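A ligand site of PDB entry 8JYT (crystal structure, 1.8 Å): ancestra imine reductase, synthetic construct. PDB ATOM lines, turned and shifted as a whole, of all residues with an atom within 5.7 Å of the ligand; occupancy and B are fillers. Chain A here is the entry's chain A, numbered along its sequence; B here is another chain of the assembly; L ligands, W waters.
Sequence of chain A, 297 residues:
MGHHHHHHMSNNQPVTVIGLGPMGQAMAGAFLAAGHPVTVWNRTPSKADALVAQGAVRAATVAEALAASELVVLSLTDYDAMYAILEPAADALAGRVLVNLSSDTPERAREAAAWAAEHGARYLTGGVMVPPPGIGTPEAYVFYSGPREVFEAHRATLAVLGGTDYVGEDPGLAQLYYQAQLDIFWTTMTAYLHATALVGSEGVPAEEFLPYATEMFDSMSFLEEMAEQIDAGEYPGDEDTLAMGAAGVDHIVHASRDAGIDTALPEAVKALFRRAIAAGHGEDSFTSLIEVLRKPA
Water W5 lies within hydrogen-bond range of O9 of the ligand (2.6 Å), N of Gly 21 (2.8 Å), N of Gly 24 (2.9 Å) and O of Ser 75 (3.0 Å). Water W2 lies within hydrogen-bond range of O11 of the ligand, O of Leu 101 and OG of Ser 75. Water W1 lies within hydrogen-bond range of the side-chain amide oxygen (OD1) of Asn 42 (2.9 Å), the backbone NH (N) of Arg 43 (2.9 Å) and a nitrogen (N5) of the ligand (3.0 Å).
The backbone NH of Leu 20 is in hydrogen-bond range of the side-chain amide oxygen of Asn 42 (3.1 Å). OG of Ser 102 lies within hydrogen-bond range of N of Leu 76, 3.0 Å away. OG of Ser 75 sits at hydrogen-bond distance from N of Gly 24. The backbone carbonyl oxygen (O) of Trp 41 lies within hydrogen-bond range of the backbone NH (N) of Gly 19, at 3.1 Å. The side-chain hydroxyl of Tyr 178 sits at hydrogen-bond distance from the side-chain hydroxyl of Ser 103 (3.2 Å). N of Ala 81 is in hydrogen-bond range of OD1 of Asp 78 (2.9 Å). O of Thr 44 is in hydrogen-bond range of ND2 of Asn 42 (2.9 Å).
NZ of Lys 47 is in salt-bridge range of O17 of the ligand, 2.7 Å away. The side-chain hydroxyl (OG1) of Thr 77 is in hydrogen-bond range of an oxygen (O2) of the ligand, at 3.3 Å. An oxygen (O15) of the ligand is in hydrogen-bond range of the backbone NH of Thr 44 (3.0 Å). O of Thr 77 is in hydrogen-bond range of O12 of the ligand (2.7 Å). O5 of the ligand sits at hydrogen-bond distance from N of Gly 21 (3.4 Å). An oxygen (O5) of the ligand is in hydrogen-bond range of the side-chain amide oxygen (OD1) of Asn 42 (2.7 Å). The backbone NH of Thr 77 is in hydrogen-bond range of an oxygen (O4) of the ligand (3.3 Å). N of Leu 20 sits at hydrogen-bond distance from O5 of the ligand, at 3.1 Å. The guanidinium group of Arg 43 is in salt-bridge range of an oxygen (O16) of the ligand. The backbone NH of Ser 103 sits at hydrogen-bond distance from an oxygen (O12) of the ligand. An oxygen (O15) of the ligand lies within hydrogen-bond range of the side-chain hydroxyl (OG1) of Thr 44, 2.9 Å away. An oxygen (O13) of the ligand sits at hydrogen-bond distance from the side-chain hydroxyl (OG) of Ser 103 (3.2 Å). O9 of the ligand is in hydrogen-bond range of N of Met 23 (3.2 Å). O12 of the ligand lies within hydrogen-bond range of O of Leu 76, 2.7 Å away.
An oxygen (O9) of the ligand lies close to the backbone nitrogen (N) of Pro 22. Merely in contact with the ligand: Val 128 (3.2 Å), Val 130 (3.2 Å), Ile 85 (3.3 Å), Pro 132 (3.4 Å), Gly 19 (3.5 Å), Ser 75 (3.5 Å), Pro 131 (3.5 Å), Ala 81 (3.5 Å), Tyr 178 (3.7 Å), Ser 102 (3.8 Å) and Leu 101 (3.96 Å). Hydrophobic or aromatic side chains that line the ligand: Pro 22, Met 23, Leu 76, Ala 81, Ile 85, Pro 131 and Pro 132. Of the 30 residues printed, 22 come within 4 Å of the ligand. The nearest printed residue that does not touch the ligand is Met 244 of chain B (4.2 Å).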
ATOM      1  N   GLY A  19      10.848   2.318  24.493  1.00  0.00           N
ATOM      2  CA  GLY A  19       9.440   2.601  24.320  1.00  0.00           C
ATOM      3  C   GLY A  19       9.149   2.843  22.859  1.00  0.00           C
ATOM      4  O   GLY A  19       9.536   3.870  22.299  1.00  0.00           O
ATOM      5  N   LEU A  20       8.490   1.884  22.213  1.00  0.00           N
ATOM      6  CA  LEU A  20       8.206   1.943  20.786  1.00  0.00           C
ATOM      7  C   LEU A  20       6.699   1.903  20.550  1.00  0.00           C
ATOM      8  O   LEU A  20       6.194   1.257  19.633  1.00  0.00           O
ATOM      9  CB  LEU A  20       8.929   0.811  20.060  1.00  0.00           C
ATOM     10  CG  LEU A  20      10.436   1.002  19.875  1.00  0.00           C
ATOM     11  CD1 LEU A  20      10.962   0.010  18.801  1.00  0.00           C
ATOM     12  CD2 LEU A  20      10.799   2.430  19.487  1.00  0.00           C
ATOM     13  N   GLY A  21       5.953   2.593  21.393  1.00  0.00           N
ATOM     14  CA  GLY A  21       4.585   2.900  21.062  1.00  0.00           C
ATOM     15  C   GLY A  21       4.556   3.905  19.933  1.00  0.00           C
ATOM     16  O   GLY A  21       5.598   4.217  19.329  1.00  0.00           O
ATOM     17  N   PRO A  22       3.368   4.440  19.612  1.00  0.00           N
ATOM     18  CA  PRO A  22       3.280   5.427  18.526  1.00  0.00           C
ATOM     19  C   PRO A  22       4.291   6.554  18.646  1.00  0.00           C
ATOM     20  O   PRO A  22       4.915   6.931  17.648  1.00  0.00           O
ATOM     21  CB  PRO A  22       1.832   5.927  18.634  1.00  0.00           C
ATOM     22  CG  PRO A  22       1.092   4.688  19.134  1.00  0.00           C
ATOM     23  CD  PRO A  22       2.040   4.139  20.181  1.00  0.00           C
ATOM     24  N   MET A  23       4.484   7.117  19.848  1.00  0.00           N
ATOM     25  CA  MET A  23       5.379   8.255  20.002  1.00  0.00           C
ATOM     26  C   MET A  23       6.854   7.851  19.896  1.00  0.00           C
ATOM     27  O   MET A  23       7.643   8.523  19.229  1.00  0.00           O
ATOM     28  CB  MET A  23       5.143   8.961  21.343  1.00  0.00           C
ATOM     29  CG  MET A  23       3.789   9.635  21.464  1.00  0.00           C
ATOM     30  SD  MET A  23       3.689  11.231  20.605  1.00  0.00           S
ATOM     31  CE  MET A  23       4.959  12.164  21.451  1.00  0.00           C
ATOM     32  N   GLY A  24       7.240   6.785  20.603  1.00  0.00           N
ATOM     33  CA  GLY A  24       8.625   6.342  20.548  1.00  0.00           C
ATOM     34  C   GLY A  24       9.036   5.922  19.147  1.00  0.00           C
ATOM     35  O   GLY A  24      10.162   6.204  18.718  1.00  0.00           O
ATOM     36  N   TRP A  41      14.666  -0.370  22.019  1.00  0.00           N
ATOM     37  CA  TRP A  41      14.235  -1.514  22.811  1.00  0.00           C
ATOM     38  C   TRP A  41      12.748  -1.362  23.132  1.00  0.00           C
ATOM     39  O   TRP A  41      12.273  -0.247  23.399  1.00  0.00           O
ATOM     40  CB  TRP A  41      15.061  -1.674  24.098  1.00  0.00           C
ATOM     41  CG  TRP A  41      14.673  -2.893  24.895  1.00  0.00           C
ATOM     42  CD1 TRP A  41      15.330  -4.101  24.939  1.00  0.00           C
ATOM     43  CD2 TRP A  41      13.533  -3.029  25.767  1.00  0.00           C
ATOM     44  NE1 TRP A  41      14.659  -4.974  25.751  1.00  0.00           N
ATOM     45  CE2 TRP A  41      13.561  -4.343  26.283  1.00  0.00           C
ATOM     46  CE3 TRP A  41      12.500  -2.177  26.154  1.00  0.00           C
ATOM     47  CZ2 TRP A  41      12.608  -4.822  27.164  1.00  0.00           C
ATOM     48  CZ3 TRP A  41      11.544  -2.658  27.018  1.00  0.00           C
ATOM     49  CH2 TRP A  41      11.598  -3.960  27.515  1.00  0.00           C
ATOM     50  N   ASN A  42      12.022  -2.477  23.103  1.00  0.00           N
ATOM     51  CA  ASN A  42      10.622  -2.456  23.467  1.00  0.00           C
ATOM     52  C   ASN A  42      10.225  -3.821  24.020  1.00  0.00           C
ATOM     53  O   ASN A  42      10.710  -4.863  23.561  1.00  0.00           O
ATOM     54  CB  ASN A  42       9.732  -2.107  22.263  1.00  0.00           C
ATOM     55  CG  ASN A  42       8.306  -1.818  22.676  1.00  0.00           C
ATOM     56  OD1 ASN A  42       8.084  -0.949  23.503  1.00  0.00           O
ATOM     57  ND2 ASN A  42       7.352  -2.537  22.123  1.00  0.00           N
ATOM     58  N   ARG A  43       9.324  -3.810  25.004  1.00  0.00           N
ATOM     59  CA  ARG A  43       8.868  -5.061  25.599  1.00  0.00           C
ATOM     60  C   ARG A  43       8.254  -5.974  24.533  1.00  0.00           C
ATOM     61  O   ARG A  43       8.399  -7.202  24.593  1.00  0.00           O
ATOM     62  CB  ARG A  43       7.846  -4.770  26.697  1.00  0.00           C
ATOM     63  CG  ARG A  43       6.764  -5.825  26.861  1.00  0.00           C
ATOM     64  CD  ARG A  43       5.815  -5.425  28.006  1.00  0.00           C
ATOM     65  NE  ARG A  43       5.016  -4.251  27.638  1.00  0.00           N
ATOM     66  CZ  ARG A  43       3.934  -3.853  28.284  1.00  0.00           C
ATOM     67  NH1 ARG A  43       3.527  -4.450  29.385  1.00  0.00           N
ATOM     68  NH2 ARG A  43       3.246  -2.818  27.814  1.00  0.00           N
ATOM     69  N   THR A  44       7.579  -5.395  23.538  1.00  0.00           N
ATOM     70  CA  THR A  44       7.019  -6.114  22.402  1.00  0.00           C
ATOM     71  C   THR A  44       7.949  -5.912  21.203  1.00  0.00           C
ATOM     72  O   THR A  44       7.827  -4.890  20.510  1.00  0.00           O
ATOM     73  CB  THR A  44       5.610  -5.632  22.092  1.00  0.00           C
ATOM     74  OG1 THR A  44       4.756  -5.870  23.214  1.00  0.00           O
ATOM     75  CG2 THR A  44       5.058  -6.332  20.870  1.00  0.00           C
ATOM     76  N   LYS A  47       7.452  -4.315  17.392  1.00  0.00           N
ATOM     77  CA  LYS A  47       7.231  -2.907  17.070  1.00  0.00           C
ATOM     78  C   LYS A  47       8.506  -2.202  16.632  1.00  0.00           C
ATOM     79  O   LYS A  47       8.432  -1.023  16.268  1.00  0.00           O
ATOM     80  CB  LYS A  47       6.625  -2.189  18.273  1.00  0.00           C
ATOM     81  CG  LYS A  47       5.485  -2.948  18.933  1.00  0.00           C
ATOM     82  CD  LYS A  47       4.379  -2.004  19.383  1.00  0.00           C
ATOM     83  CE  LYS A  47       3.574  -2.607  20.526  1.00  0.00           C
ATOM     84  NZ  LYS A  47       2.968  -1.552  21.431  1.00  0.00           N
ATOM     85  N   SER A  75       9.986   6.783  26.144  1.00  0.00           N
ATOM     86  CA  SER A  75       8.641   7.161  25.696  1.00  0.00           C
ATOM     87  C   SER A  75       7.727   5.983  26.076  1.00  0.00           C
ATOM     88  O   SER A  75       7.502   5.068  25.279  1.00  0.00           O
ATOM     89  CB  SER A  75       8.584   7.469  24.208  1.00  0.00           C
ATOM     90  OG  SER A  75       7.260   7.888  23.853  1.00  0.00           O
ATOM     91  N   LEU A  76       7.191   6.027  27.294  1.00  0.00           N
ATOM     92  CA  LEU A  76       6.431   4.934  27.873  1.00  0.00           C
ATOM     93  C   LEU A  76       5.116   5.475  28.418  1.00  0.00           C
ATOM     94  O   LEU A  76       4.915   6.687  28.495  1.00  0.00           O
ATOM     95  CB  LEU A  76       7.209   4.232  28.996  1.00  0.00           C
ATOM     96  CG  LEU A  76       8.470   3.482  28.563  1.00  0.00           C
ATOM     97  CD1 LEU A  76       9.391   3.271  29.772  1.00  0.00           C
ATOM     98  CD2 LEU A  76       8.103   2.157  27.926  1.00  0.00           C
ATOM     99  N   THR A  77       4.205   4.552  28.726  1.00  0.00           N
ATOM    100  CA  THR A  77       2.886   4.936  29.229  1.00  0.00           C
ATOM    101  C   THR A  77       3.002   5.876  30.410  1.00  0.00           C
ATOM    102  O   THR A  77       2.505   7.009  30.379  1.00  0.00           O
ATOM    103  CB  THR A  77       2.093   3.680  29.604  1.00  0.00           C
ATOM    104  OG1 THR A  77       1.726   2.961  28.414  1.00  0.00           O
ATOM    105  CG2 THR A  77       0.834   4.047  30.374  1.00  0.00           C
ATOM    106  N   ASP A  78       3.669   5.425  31.477  1.00  0.00           N
ATOM    107  CA  ASP A  78       3.844   6.206  32.686  1.00  0.00           C
ATOM    108  C   ASP A  78       5.214   5.879  33.284  1.00  0.00           C
ATOM    109  O   ASP A  78       5.994   5.107  32.725  1.00  0.00           O
ATOM    110  CB  ASP A  78       2.710   5.957  33.703  1.00  0.00           C
ATOM    111  CG  ASP A  78       2.514   4.487  34.034  1.00  0.00           C
ATOM    112  OD1 ASP A  78       3.499   3.710  33.980  1.00  0.00           O
ATOM    113  OD2 ASP A  78       1.378   4.091  34.363  1.00  0.00           O
ATOM    114  N   ASP A  80       5.666   4.196  36.008  1.00  0.00           N
ATOM    115  CA  ASP A  80       5.663   2.814  36.476  1.00  0.00           C
ATOM    116  C   ASP A  80       6.266   1.895  35.422  1.00  0.00           C
ATOM    117  O   ASP A  80       6.998   0.963  35.750  1.00  0.00           O
ATOM    118  CB  ASP A  80       4.239   2.374  36.799  1.00  0.00           C
ATOM    119  CG  ASP A  80       3.702   3.030  38.066  1.00  0.00           C
ATOM    120  OD1 ASP A  80       4.454   3.129  39.059  1.00  0.00           O
ATOM    121  OD2 ASP A  80       2.522   3.440  38.074  1.00  0.00           O
ATOM    122  N   ALA A  81       5.928   2.125  34.148  1.00  0.00           N
ATOM    123  CA  ALA A  81       6.527   1.359  33.057  1.00  0.00           C
ATOM    124  C   ALA A  81       8.046   1.542  33.029  1.00  0.00           C
ATOM    125  O   ALA A  81       8.785   0.591  32.756  1.00  0.00           O
ATOM    126  CB  ALA A  81       5.906   1.796  31.729  1.00  0.00           C
ATOM    127  N   ALA A  84       9.633  -0.530  35.924  1.00  0.00           N
ATOM    128  CA  ALA A  84       9.553  -1.940  35.571  1.00  0.00           C
ATOM    129  C   ALA A  84      10.628  -2.323  34.548  1.00  0.00           C
ATOM    130  O   ALA A  84      11.219  -3.398  34.627  1.00  0.00           O
ATOM    131  CB  ALA A  84       8.162  -2.273  35.040  1.00  0.00           C
ATOM    132  N   ILE A  85      10.884  -1.436  33.590  1.00  0.00           N
ATOM    133  CA  ILE A  85      11.847  -1.721  32.531  1.00  0.00           C
ATOM    134  C   ILE A  85      13.279  -1.541  33.022  1.00  0.00           C
ATOM    135  O   ILE A  85      14.162  -2.366  32.750  1.00  0.00           O
ATOM    136  CB  ILE A  85      11.566  -0.829  31.313  1.00  0.00           C
ATOM    137  CG1 ILE A  85      10.311  -1.290  30.568  1.00  0.00           C
ATOM    138  CG2 ILE A  85      12.750  -0.806  30.355  1.00  0.00           C
ATOM    139  CD1 ILE A  85       9.662  -0.194  29.755  1.00  0.00           C
ATOM    140  N   LEU A 101      10.375  11.386  28.277  1.00  0.00           N
ATOM    141  CA  LEU A 101       9.339  12.132  27.582  1.00  0.00           C
ATOM    142  C   LEU A 101       7.964  11.536  27.876  1.00  0.00           C
ATOM    143  O   LEU A 101       6.996  11.840  27.157  1.00  0.00           O
ATOM    144  CB  LEU A 101       9.628  12.137  26.081  1.00  0.00           C
ATOM    145  CG  LEU A 101      11.008  12.673  25.733  1.00  0.00           C
ATOM    146  CD1 LEU A 101      11.241  12.722  24.209  1.00  0.00           C
ATOM    147  CD2 LEU A 101      11.267  14.042  26.304  1.00  0.00           C
ATOM    148  N   SER A 102       7.856  10.756  28.950  1.00  0.00           N
ATOM    149  CA  SER A 102       6.612  10.111  29.318  1.00  0.00           C
ATOM    150  C   SER A 102       5.793  11.048  30.204  1.00  0.00           C
ATOM    151  O   SER A 102       6.355  11.795  31.006  1.00  0.00           O
ATOM    152  CB  SER A 102       6.882   8.814  30.086  1.00  0.00           C
ATOM    153  OG  SER A 102       7.856   8.026  29.410  1.00  0.00           O
ATOM    154  N   SER A 103       4.475  10.984  30.070  1.00  0.00           N
ATOM    155  CA  SER A 103       3.591  11.859  30.827  1.00  0.00           C
ATOM    156  C   SER A 103       3.399  11.292  32.228  1.00  0.00           C
ATOM    157  O   SER A 103       3.054  10.117  32.387  1.00  0.00           O
ATOM    158  CB  SER A 103       2.253  11.982  30.101  1.00  0.00           C
ATOM    159  OG  SER A 103       2.441  12.719  28.898  1.00  0.00           O
ATOM    160  N   VAL A 128       6.006  16.464  25.766  1.00  0.00           N
ATOM    161  CA  VAL A 128       5.854  16.567  24.321  1.00  0.00           C
ATOM    162  C   VAL A 128       4.453  17.037  23.981  1.00  0.00           C
ATOM    163  O   VAL A 128       3.462  16.373  24.285  1.00  0.00           O
ATOM    164  CB  VAL A 128       6.155  15.223  23.631  1.00  0.00           C
ATOM    165  CG1 VAL A 128       6.091  15.395  22.110  1.00  0.00           C
ATOM    166  CG2 VAL A 128       7.497  14.665  24.055  1.00  0.00           C
ATOM    167  N   MET A 129       4.373  18.172  23.292  1.00  0.00           N
ATOM    168  CA  MET A 129       3.120  18.856  23.040  1.00  0.00           C
ATOM    169  C   MET A 129       2.589  18.627  21.628  1.00  0.00           C
ATOM    170  O   MET A 129       1.908  19.502  21.095  1.00  0.00           O
ATOM    171  CB  MET A 129       3.294  20.346  23.296  1.00  0.00           C
ATOM    172  CG  MET A 129       3.415  20.772  24.755  1.00  0.00           C
ATOM    173  SD  MET A 129       2.140  20.027  25.788  1.00  0.00           S
ATOM    174  CE  MET A 129       0.659  20.721  25.099  1.00  0.00           C
ATOM    175  N   VAL A 130       2.900  17.482  21.029  1.00  0.00           N
ATOM    176  CA  VAL A 130       2.390  17.116  19.702  1.00  0.00           C
ATOM    177  C   VAL A 130       2.064  15.638  19.680  1.00  0.00           C
ATOM    178  O   VAL A 130       2.680  14.829  20.413  1.00  0.00           O
ATOM    179  CB  VAL A 130       3.411  17.422  18.588  1.00  0.00           C
ATOM    180  CG1 VAL A 130       3.431  18.899  18.273  1.00  0.00           C
ATOM    181  CG2 VAL A 130       4.776  16.936  18.972  1.00  0.00           C
ATOM    182  N   PRO A 131       1.129  15.235  18.833  1.00  0.00           N
ATOM    183  CA  PRO A 131       0.889  13.809  18.607  1.00  0.00           C
ATOM    184  C   PRO A 131       1.996  13.210  17.746  1.00  0.00           C
ATOM    185  O   PRO A 131       2.844  13.940  17.203  1.00  0.00           O
ATOM    186  CB  PRO A 131      -0.471  13.790  17.886  1.00  0.00           C
ATOM    187  CG  PRO A 131      -0.390  15.041  17.050  1.00  0.00           C
ATOM    188  CD  PRO A 131       0.281  16.071  17.958  1.00  0.00           C
ATOM    189  N   PRO A 132       2.037  11.887  17.610  1.00  0.00           N
ATOM    190  CA  PRO A 132       3.169  11.247  16.913  1.00  0.00           C
ATOM    191  C   PRO A 132       3.380  11.799  15.511  1.00  0.00           C
ATOM    192  O   PRO A 132       4.525  12.028  15.095  1.00  0.00           O
ATOM    193  CB  PRO A 132       2.777   9.763  16.887  1.00  0.00           C
ATOM    194  CG  PRO A 132       1.946   9.582  18.136  1.00  0.00           C
ATOM    195  CD  PRO A 132       1.141  10.905  18.245  1.00  0.00           C
ATOM    196  N   TYR A 178       3.546  20.973  31.109  1.00  0.00           N
ATOM    197  CA  TYR A 178       2.774  20.070  30.243  1.00  0.00           C
ATOM    198  C   TYR A 178       1.388  19.797  30.833  1.00  0.00           C
ATOM    199  O   TYR A 178       0.370  19.908  30.124  1.00  0.00           O
ATOM    200  CB  TYR A 178       3.589  18.766  30.018  1.00  0.00           C
ATOM    201  CG  TYR A 178       2.832  17.677  29.273  1.00  0.00           C
ATOM    202  CD1 TYR A 178       2.890  17.611  27.899  1.00  0.00           C
ATOM    203  CD2 TYR A 178       2.095  16.711  29.936  1.00  0.00           C
ATOM    204  CE1 TYR A 178       2.205  16.639  27.195  1.00  0.00           C
ATOM    205  CE2 TYR A 178       1.399  15.743  29.251  1.00  0.00           C
ATOM    206  CZ  TYR A 178       1.464  15.703  27.861  1.00  0.00           C
ATOM    207  OH  TYR A 178       0.766  14.748  27.116  1.00  0.00           O
ATOM    208  N   GLU B 239      -6.308   8.469  16.919  1.00  0.00           N
ATOM    209  CA  GLU B 239      -5.138   9.060  17.544  1.00  0.00           C
ATOM    210  C   GLU B 239      -5.431   9.694  18.896  1.00  0.00           C
ATOM    211  O   GLU B 239      -4.505  10.184  19.554  1.00  0.00           O
ATOM    212  CB  GLU B 239      -4.529  10.136  16.618  1.00  0.00           C
ATOM    213  CG  GLU B 239      -5.568  11.027  15.892  1.00  0.00           C
ATOM    214  CD  GLU B 239      -6.235  10.360  14.730  1.00  0.00           C
ATOM    215  OE1 GLU B 239      -5.909   9.187  14.556  1.00  0.00           O
ATOM    216  OE2 GLU B 239      -7.112  10.945  14.056  1.00  0.00           O
ATOM    217  N   MET B 244      -7.387   7.668  26.535  1.00  0.00           N
ATOM    218  CA  MET B 244      -6.166   8.454  26.590  1.00  0.00           C
ATOM    219  C   MET B 244      -6.378   9.746  27.368  1.00  0.00           C
ATOM    220  O   MET B 244      -5.601  10.087  28.257  1.00  0.00           O
ATOM    221  CB  MET B 244      -5.686   8.755  25.160  1.00  0.00           C
ATOM    222  CG  MET B 244      -4.904   7.618  24.518  1.00  0.00           C
ATOM    223  SD  MET B 244      -4.866   7.725  22.718  1.00  0.00           S
ATOM    224  CE  MET B 244      -3.629   9.003  22.469  1.00  0.00           C
HETATM  225  P1  LIG L   1       1.525   4.518  25.153  1.00  0.00           P
HETATM  226  O1  LIG L   1       0.523   3.411  25.070  1.00  0.00           O
HETATM  227  O2  LIG L   1       1.454   5.459  26.299  1.00  0.00           O
HETATM  228  O3  LIG L   1       2.995   3.919  25.067  1.00  0.00           O
HETATM  229  C1  LIG L   1       3.130   2.519  25.387  1.00  0.00           C
HETATM  230  C2  LIG L   1       4.594   2.183  25.466  1.00  0.00           C
HETATM  231  O4  LIG L   1       4.928   1.928  26.850  1.00  0.00           O
HETATM  232  C3  LIG L   1       5.009   0.912  24.718  1.00  0.00           C
HETATM  233  O5  LIG L   1       6.380   0.963  24.347  1.00  0.00           O
HETATM  234  C4  LIG L   1       4.689  -0.126  25.780  1.00  0.00           C
HETATM  235  O6  LIG L   1       5.318  -1.395  25.710  1.00  0.00           O
HETATM  236  C5  LIG L   1       5.309   0.581  26.976  1.00  0.00           C
HETATM  237  N1  LIG L   1       4.845   0.039  28.249  1.00  0.00           N
HETATM  238  C6  LIG L   1       3.662   0.283  28.875  1.00  0.00           C
HETATM  239  N2  LIG L   1       3.520  -0.365  29.996  1.00  0.00           N
HETATM  240  C7  LIG L   1       4.692  -1.094  30.109  1.00  0.00           C
HETATM  241  C8  LIG L   1       5.169  -1.986  31.089  1.00  0.00           C
HETATM  242  N3  LIG L   1       4.483  -2.305  32.187  1.00  0.00           N
HETATM  243  N4  LIG L   1       6.381  -2.539  30.900  1.00  0.00           N
HETATM  244  C9  LIG L   1       7.067  -2.221  29.801  1.00  0.00           C
HETATM  245  N5  LIG L   1       6.727  -1.391  28.819  1.00  0.00           N
HETATM  246  C10 LIG L   1       5.516  -0.861  29.027  1.00  0.00           C
HETATM  247  O7  LIG L   1       1.463   5.344  23.788  1.00  0.00           O
HETATM  248  P2  LIG L   1       2.351   6.524  23.183  1.00  0.00           P
HETATM  249  O8  LIG L   1       1.515   7.318  22.245  1.00  0.00           O
HETATM  250  O9  LIG L   1       3.615   5.930  22.669  1.00  0.00           O
HETATM  251  O10 LIG L   1       2.655   7.394  24.489  1.00  0.00           O
HETATM  252  C11 LIG L   1       3.988   7.484  25.018  1.00  0.00           C
HETATM  253  C12 LIG L   1       4.007   8.511  26.121  1.00  0.00           C
HETATM  254  O11 LIG L   1       4.002   9.827  25.531  1.00  0.00           O
HETATM  255  C13 LIG L   1       2.799   8.469  27.074  1.00  0.00           C
HETATM  256  O12 LIG L   1       3.157   8.767  28.406  1.00  0.00           O
HETATM  257  C14 LIG L   1       1.869   9.550  26.516  1.00  0.00           C
HETATM  258  O13 LIG L   1       1.095  10.183  27.523  1.00  0.00           O
HETATM  259  C15 LIG L   1       2.878  10.561  25.969  1.00  0.00           C
HETATM  260  N6  LIG L   1       2.384  11.366  24.829  1.00  0.00           N
HETATM  261  C16 LIG L   1       1.601  10.789  23.852  1.00  0.00           C
HETATM  262  C17 LIG L   1       1.151  11.553  22.785  1.00  0.00           C
HETATM  263  C18 LIG L   1       0.292  10.933  21.731  1.00  0.00           C
HETATM  264  O14 LIG L   1       0.359   9.714  21.516  1.00  0.00           O
HETATM  265  N7  LIG L   1      -0.533  11.719  21.058  1.00  0.00           N
HETATM  266  C19 LIG L   1       1.507  12.896  22.696  1.00  0.00           C
HETATM  267  C20 LIG L   1       2.301  13.447  23.674  1.00  0.00           C
HETATM  268  C21 LIG L   1       2.742  12.687  24.730  1.00  0.00           C
HETATM  269  P3  LIG L   1       4.677  -2.344  24.588  1.00  0.00           P
HETATM  270  O15 LIG L   1       5.602  -3.502  24.647  1.00  0.00           O
HETATM  271  O16 LIG L   1       3.246  -2.709  24.829  1.00  0.00           O
HETATM  272  O17 LIG L   1       4.846  -1.537  23.358  1.00  0.00           O
HETATM  273  O   HOH W   1       8.364  -1.360  26.310  1.00  0.00           O
HETATM  274  O   HOH W   2       6.541  10.596  24.682  1.00  0.00           O
HETATM  275  O   HOH W   3       7.689  -4.852  31.580  1.00  0.00           O
HETATM  276  O   HOH W   4      -0.752   5.989  21.614  1.00  0.00           O
HETATM  277  O   HOH W   5       6.070   5.082  22.633  1.00  0.00           O
HETATM  278  O   HOH W   6      -1.397   7.908  19.400  1.00  0.00           O
HETATM  279  O   HOH W   7       1.102  -0.915  24.339  1.00  0.00           O
